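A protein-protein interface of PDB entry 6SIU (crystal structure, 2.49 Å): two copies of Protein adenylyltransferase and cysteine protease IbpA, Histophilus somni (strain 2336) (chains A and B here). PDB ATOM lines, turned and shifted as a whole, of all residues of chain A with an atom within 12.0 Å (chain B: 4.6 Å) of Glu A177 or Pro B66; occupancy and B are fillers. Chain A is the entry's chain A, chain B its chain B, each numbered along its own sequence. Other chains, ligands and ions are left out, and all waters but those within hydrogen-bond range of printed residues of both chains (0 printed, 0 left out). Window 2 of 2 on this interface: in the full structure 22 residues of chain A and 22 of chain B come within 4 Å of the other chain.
The backbone NH (N) of Glu A177 lies within hydrogen-bond range of the backbone carbonyl oxygen (O) of Ser B63, 2.7 Å away.
Gly A176 touches Ser B63.
CG of Glu A177 touches O of Leu B65 (3.1 Å).
Glu A177 touches Pro B66 (CG to CA, 3.5 Å).
Glu A177 touches Phe B68.
CA of Gly A178 touches OD1 of Asp B69 (3.96 Å).
Of the printed residues of chain B, Gly A176 touches Ser B63.
Of the printed residues of chain B, Gly A178 touches Asp B69.
Leu B65 touches one residue of chain A.
Printed residues of chain A within 4 Å of Pro B66: Glu A177.
No residue of chain A comes within 4 Å of Glu B67.
Printed residues of chain A within 4 Å of Phe B68: Glu A177.
The nearest residue of chain A that does not touch Pro B66 is Gly A178 (6.4 Å).
The nearest printed residue of chain B that does not touch Gly A178 is Phe B68 (4.02 Å).
Of the 7 printed residues of chain B, 5 touch a printed residue of chain A.
Printed residues of chain B that touch a printed residue of chain A: Ser B63, Leu B65, Pro B66, Phe B68 and Asp B69.
Hydrophobic or aromatic side chains of chain B that line the printed part of chain A: Phe B68.
Among the printed residues, 6 pairs touch across the chains.
Among the printed residues, no Asp or Glu carboxylate lies within 4 Å of a Lys or Arg side-chain nitrogen of the other chain.
No position is printed for both chains.
Of the 6 pairs that touch across the chains among the printed residues, none has its exchanged pair printed and touching as well.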
ATOM      1  N   GLN A 142     -16.184  23.930   8.496  1.00  0.00           N
ATOM      2  CA  GLN A 142     -17.624  23.694   8.551  1.00  0.00           C
ATOM      3  C   GLN A 142     -18.318  24.233   7.304  1.00  0.00           C
ATOM      4  O   GLN A 142     -19.199  23.572   6.741  1.00  0.00           O
ATOM      5  CB  GLN A 142     -18.206  24.331   9.813  1.00  0.00           C
ATOM      6  CG  GLN A 142     -17.776  23.656  11.102  1.00  0.00           C
ATOM      7  CD  GLN A 142     -18.310  24.353  12.337  1.00  0.00           C
ATOM      8  OE1 GLN A 142     -18.133  25.558  12.508  1.00  0.00           O
ATOM      9  NE2 GLN A 142     -18.970  23.596  13.204  1.00  0.00           N
ATOM     10  N   HIS A 169     -28.569  27.073   6.004  1.00  0.00           N
ATOM     11  CA  HIS A 169     -28.397  26.521   7.337  1.00  0.00           C
ATOM     12  C   HIS A 169     -26.973  26.011   7.537  1.00  0.00           C
ATOM     13  O   HIS A 169     -26.371  26.226   8.597  1.00  0.00           O
ATOM     14  CB  HIS A 169     -29.419  25.416   7.565  1.00  0.00           C
ATOM     15  CG  HIS A 169     -29.274  24.730   8.882  1.00  0.00           C
ATOM     16  ND1 HIS A 169     -29.690  25.301  10.066  1.00  0.00           N
ATOM     17  CD2 HIS A 169     -28.746  23.526   9.204  1.00  0.00           C
ATOM     18  CE1 HIS A 169     -29.427  24.469  11.059  1.00  0.00           C
ATOM     19  NE2 HIS A 169     -28.852  23.387  10.564  1.00  0.00           N
ATOM     20  N   GLY A 170     -26.410  25.362   6.515  1.00  0.00           N
ATOM     21  CA  GLY A 170     -25.046  24.873   6.611  1.00  0.00           C
ATOM     22  C   GLY A 170     -24.017  25.975   6.762  1.00  0.00           C
ATOM     23  O   GLY A 170     -22.970  25.770   7.382  1.00  0.00           O
ATOM     24  N   ARG A 172     -24.426  28.606   8.510  1.00  0.00           N
ATOM     25  CA  ARG A 172     -24.669  29.257   9.797  1.00  0.00           C
ATOM     26  C   ARG A 172     -24.408  28.258  10.918  1.00  0.00           C
ATOM     27  O   ARG A 172     -25.339  27.821  11.609  1.00  0.00           O
ATOM     28  CB  ARG A 172     -26.095  29.797   9.876  1.00  0.00           C
ATOM     29  CG  ARG A 172     -26.409  30.823   8.823  1.00  0.00           C
ATOM     30  CD  ARG A 172     -27.896  30.836   8.492  1.00  0.00           C
ATOM     31  NE  ARG A 172     -28.724  31.257   9.616  1.00  0.00           N
ATOM     32  CZ  ARG A 172     -30.035  31.450   9.534  1.00  0.00           C
ATOM     33  NH1 ARG A 172     -30.721  31.833  10.602  1.00  0.00           N
ATOM     34  NH2 ARG A 172     -30.658  31.262   8.380  1.00  0.00           N
ATOM     35  N   PRO A 173     -23.145  27.877  11.130  1.00  0.00           N
ATOM     36  CA  PRO A 173     -22.832  26.880  12.159  1.00  0.00           C
ATOM     37  C   PRO A 173     -22.542  27.451  13.534  1.00  0.00           C
ATOM     38  O   PRO A 173     -22.419  26.675  14.490  1.00  0.00           O
ATOM     39  CB  PRO A 173     -21.583  26.206  11.585  1.00  0.00           C
ATOM     40  CG  PRO A 173     -20.880  27.329  10.893  1.00  0.00           C
ATOM     41  CD  PRO A 173     -21.950  28.254  10.358  1.00  0.00           C
ATOM     42  N   ASP A 174     -22.424  28.769  13.663  1.00  0.00           N
ATOM     43  CA  ASP A 174     -22.122  29.405  14.937  1.00  0.00           C
ATOM     44  C   ASP A 174     -23.356  30.024  15.584  1.00  0.00           C
ATOM     45  O   ASP A 174     -23.227  30.912  16.433  1.00  0.00           O
ATOM     46  CB  ASP A 174     -21.034  30.464  14.751  1.00  0.00           C
ATOM     47  CG  ASP A 174     -19.727  29.879  14.244  1.00  0.00           C
ATOM     48  OD1 ASP A 174     -19.600  28.636  14.202  1.00  0.00           O
ATOM     49  OD2 ASP A 174     -18.824  30.666  13.885  1.00  0.00           O
ATOM     50  N   GLU A 175     -24.548  29.569  15.205  1.00  0.00           N
ATOM     51  CA  GLU A 175     -25.775  30.225  15.632  1.00  0.00           C
ATOM     52  C   GLU A 175     -26.295  29.699  16.962  1.00  0.00           C
ATOM     53  O   GLU A 175     -26.680  30.481  17.837  1.00  0.00           O
ATOM     54  CB  GLU A 175     -26.859  30.045  14.573  1.00  0.00           C
ATOM     55  CG  GLU A 175     -26.826  31.051  13.467  1.00  0.00           C
ATOM     56  CD  GLU A 175     -28.092  30.996  12.660  1.00  0.00           C
ATOM     57  OE1 GLU A 175     -28.772  29.946  12.711  1.00  0.00           O
ATOM     58  OE2 GLU A 175     -28.420  31.996  11.994  1.00  0.00           O
ATOM     59  N   GLY A 176     -26.334  28.385  17.118  1.00  0.00           N
ATOM     60  CA  GLY A 176     -27.048  27.800  18.227  1.00  0.00           C
ATOM     61  C   GLY A 176     -28.386  27.231  17.787  1.00  0.00           C
ATOM     62  O   GLY A 176     -28.968  27.623  16.771  1.00  0.00           O
ATOM     63  N   GLU A 177     -28.881  26.291  18.577  1.00  0.00           N
ATOM     64  CA  GLU A 177     -30.056  25.542  18.179  1.00  0.00           C
ATOM     65  C   GLU A 177     -31.315  26.387  18.309  1.00  0.00           C
ATOM     66  O   GLU A 177     -31.385  27.334  19.095  1.00  0.00           O
ATOM     67  CB  GLU A 177     -30.182  24.275  19.021  1.00  0.00           C
ATOM     68  CG  GLU A 177     -28.920  23.451  19.040  1.00  0.00           C
ATOM     69  CD  GLU A 177     -28.581  22.876  17.682  1.00  0.00           C
ATOM     70  OE1 GLU A 177     -29.504  22.710  16.856  1.00  0.00           O
ATOM     71  OE2 GLU A 177     -27.389  22.590  17.438  1.00  0.00           O
ATOM     72  N   GLY A 178     -32.322  26.023  17.520  1.00  0.00           N
ATOM     73  CA  GLY A 178     -33.617  26.647  17.617  1.00  0.00           C
ATOM     74  C   GLY A 178     -33.754  27.950  16.874  1.00  0.00           C
ATOM     75  O   GLY A 178     -34.822  28.562  16.937  1.00  0.00           O
ATOM     76  N   ARG A 179     -32.721  28.392  16.170  1.00  0.00           N
ATOM     77  CA  ARG A 179     -32.804  29.651  15.448  1.00  0.00           C
ATOM     78  C   ARG A 179     -33.716  29.517  14.239  1.00  0.00           C
ATOM     79  O   ARG A 179     -33.762  28.472  13.581  1.00  0.00           O
ATOM     80  CB  ARG A 179     -31.412  30.112  15.014  1.00  0.00           C
ATOM     81  CG  ARG A 179     -30.613  30.788  16.121  1.00  0.00           C
ATOM     82  CD  ARG A 179     -31.295  32.061  16.611  1.00  0.00           C
ATOM     83  NE  ARG A 179     -30.466  32.784  17.573  1.00  0.00           N
ATOM     84  CZ  ARG A 179     -29.673  33.804  17.260  1.00  0.00           C
ATOM     85  NH1 ARG A 179     -29.608  34.231  16.004  1.00  0.00           N
ATOM     86  NH2 ARG A 179     -28.948  34.399  18.202  1.00  0.00           N
ATOM     87  N   LEU A 180     -34.467  30.579  13.965  1.00  0.00           N
ATOM     88  CA  LEU A 180     -35.311  30.615  12.782  1.00  0.00           C
ATOM     89  C   LEU A 180     -34.447  30.617  11.534  1.00  0.00           C
ATOM     90  O   LEU A 180     -33.390  31.253  11.488  1.00  0.00           O
ATOM     91  CB  LEU A 180     -36.206  31.850  12.804  1.00  0.00           C
ATOM     92  CG  LEU A 180     -37.565  31.709  13.486  1.00  0.00           C
ATOM     93  CD1 LEU A 180     -37.397  31.444  14.970  1.00  0.00           C
ATOM     94  CD2 LEU A 180     -38.407  32.951  13.262  1.00  0.00           C
ATOM     95  N   LEU A 181     -34.891  29.881  10.519  1.00  0.00           N
ATOM     96  CA  LEU A 181     -34.169  29.879   9.256  1.00  0.00           C
ATOM     97  C   LEU A 181     -34.341  31.217   8.549  1.00  0.00           C
ATOM     98  O   LEU A 181     -33.368  31.949   8.324  1.00  0.00           O
ATOM     99  CB  LEU A 181     -34.649  28.724   8.375  1.00  0.00           C
ATOM    100  CG  LEU A 181     -33.903  28.527   7.054  1.00  0.00           C
ATOM    101  CD1 LEU A 181     -32.426  28.229   7.291  1.00  0.00           C
ATOM    102  CD2 LEU A 181     -34.548  27.420   6.227  1.00  0.00           C
ATOM    103  N   ALA A 239     -32.406  34.753   7.994  1.00  0.00           N
ATOM    104  CA  ALA A 239     -32.043  35.547   9.162  1.00  0.00           C
ATOM    105  C   ALA A 239     -30.553  35.852   9.169  1.00  0.00           C
ATOM    106  O   ALA A 239     -30.136  36.955   9.545  1.00  0.00           O
ATOM    107  CB  ALA A 239     -32.454  34.824  10.444  1.00  0.00           C
ATOM    108  N   GLU A 240     -29.735  34.899   8.733  1.00  0.00           N
ATOM    109  CA  GLU A 240     -28.295  35.083   8.679  1.00  0.00           C
ATOM    110  C   GLU A 240     -27.753  34.409   7.429  1.00  0.00           C
ATOM    111  O   GLU A 240     -28.458  33.669   6.736  1.00  0.00           O
ATOM    112  CB  GLU A 240     -27.612  34.511   9.921  1.00  0.00           C
ATOM    113  CG  GLU A 240     -28.113  35.082  11.223  1.00  0.00           C
ATOM    114  CD  GLU A 240     -27.413  36.365  11.595  1.00  0.00           C
ATOM    115  OE1 GLU A 240     -26.663  36.898  10.751  1.00  0.00           O
ATOM    116  OE2 GLU A 240     -27.605  36.831  12.738  1.00  0.00           O
ATOM    117  N   SER B  63     -30.482  26.994  23.578  1.00  0.00           N
ATOM    118  CA  SER B  63     -29.867  27.012  22.261  1.00  0.00           C
ATOM    119  C   SER B  63     -28.577  26.200  22.196  1.00  0.00           C
ATOM    120  O   SER B  63     -28.109  25.916  21.088  1.00  0.00           O
ATOM    121  CB  SER B  63     -29.599  28.450  21.830  1.00  0.00           C
ATOM    122  OG  SER B  63     -28.664  29.064  22.694  1.00  0.00           O
ATOM    123  N   HIS B  64     -27.999  25.813  23.334  1.00  0.00           N
ATOM    124  CA  HIS B  64     -26.818  24.959  23.354  1.00  0.00           C
ATOM    125  C   HIS B  64     -27.153  23.479  23.388  1.00  0.00           C
ATOM    126  O   HIS B  64     -26.233  22.657  23.459  1.00  0.00           O
ATOM    127  CB  HIS B  64     -25.935  25.280  24.560  1.00  0.00           C
ATOM    128  CG  HIS B  64     -25.349  26.652  24.532  1.00  0.00           C
ATOM    129  ND1 HIS B  64     -26.029  27.760  24.991  1.00  0.00           N
ATOM    130  CD2 HIS B  64     -24.146  27.097  24.104  1.00  0.00           C
ATOM    131  CE1 HIS B  64     -25.267  28.828  24.850  1.00  0.00           C
ATOM    132  NE2 HIS B  64     -24.119  28.453  24.315  1.00  0.00           N
ATOM    133  N   LEU B  65     -28.434  23.121  23.369  1.00  0.00           N
ATOM    134  CA  LEU B  65     -28.831  21.721  23.354  1.00  0.00           C
ATOM    135  C   LEU B  65     -29.344  21.376  21.970  1.00  0.00           C
ATOM    136  O   LEU B  65     -30.264  22.053  21.481  1.00  0.00           O
ATOM    137  CB  LEU B  65     -29.909  21.449  24.395  1.00  0.00           C
ATOM    138  CG  LEU B  65     -29.446  21.053  25.796  1.00  0.00           C
ATOM    139  CD1 LEU B  65     -28.409  22.023  26.318  1.00  0.00           C
ATOM    140  CD2 LEU B  65     -30.632  20.979  26.744  1.00  0.00           C
ATOM    141  N   PRO B  66     -28.778  20.371  21.298  1.00  0.00           N
ATOM    142  CA  PRO B  66     -29.257  20.036  19.947  1.00  0.00           C
ATOM    143  C   PRO B  66     -30.726  19.659  19.895  1.00  0.00           C
ATOM    144  O   PRO B  66     -31.366  19.830  18.851  1.00  0.00           O
ATOM    145  CB  PRO B  66     -28.358  18.859  19.545  1.00  0.00           C
ATOM    146  CG  PRO B  66     -27.118  19.050  20.355  1.00  0.00           C
ATOM    147  CD  PRO B  66     -27.578  19.605  21.667  1.00  0.00           C
ATOM    148  N   GLU B  67     -31.288  19.166  20.996  1.00  0.00           N
ATOM    149  CA  GLU B  67     -32.691  18.776  21.001  1.00  0.00           C
ATOM    150  C   GLU B  67     -33.644  19.962  21.003  1.00  0.00           C
ATOM    151  O   GLU B  67     -34.857  19.754  20.893  1.00  0.00           O
ATOM    152  CB  GLU B  67     -32.973  17.917  22.221  1.00  0.00           C
ATOM    153  CG  GLU B  67     -32.992  18.712  23.497  1.00  0.00           C
ATOM    154  CD  GLU B  67     -32.485  17.909  24.660  1.00  0.00           C
ATOM    155  OE1 GLU B  67     -31.456  17.225  24.488  1.00  0.00           O
ATOM    156  OE2 GLU B  67     -33.121  17.950  25.733  1.00  0.00           O
ATOM    157  N   PHE B  68     -33.127  21.186  21.121  1.00  0.00           N
ATOM    158  CA  PHE B  68     -33.978  22.350  21.339  1.00  0.00           C
ATOM    159  C   PHE B  68     -34.934  22.571  20.173  1.00  0.00           C
ATOM    160  O   PHE B  68     -36.115  22.878  20.379  1.00  0.00           O
ATOM    161  CB  PHE B  68     -33.111  23.585  21.568  1.00  0.00           C
ATOM    162  CG  PHE B  68     -33.888  24.816  21.939  1.00  0.00           C
ATOM    163  CD1 PHE B  68     -35.084  24.719  22.634  1.00  0.00           C
ATOM    164  CD2 PHE B  68     -33.421  26.075  21.590  1.00  0.00           C
ATOM    165  CE1 PHE B  68     -35.797  25.854  22.977  1.00  0.00           C
ATOM    166  CE2 PHE B  68     -34.127  27.208  21.933  1.00  0.00           C
ATOM    167  CZ  PHE B  68     -35.314  27.099  22.623  1.00  0.00           C
ATOM    168  N   ASP B  69     -34.445  22.424  18.941  1.00  0.00           N
ATOM    169  CA  ASP B  69     -35.310  22.655  17.789  1.00  0.00           C
ATOM    170  C   ASP B  69     -36.454  21.646  17.738  1.00  0.00           C
ATOM    171  O   ASP B  69     -37.580  21.996  17.365  1.00  0.00           O
ATOM    172  CB  ASP B  69     -34.498  22.606  16.501  1.00  0.00           C
ATOM    173  CG  ASP B  69     -35.303  23.034  15.307  1.00  0.00           C
ATOM    174  OD1 ASP B  69     -35.662  24.225  15.238  1.00  0.00           O
ATOM    175  OD2 ASP B  69     -35.589  22.180  14.442  1.00  0.00           O
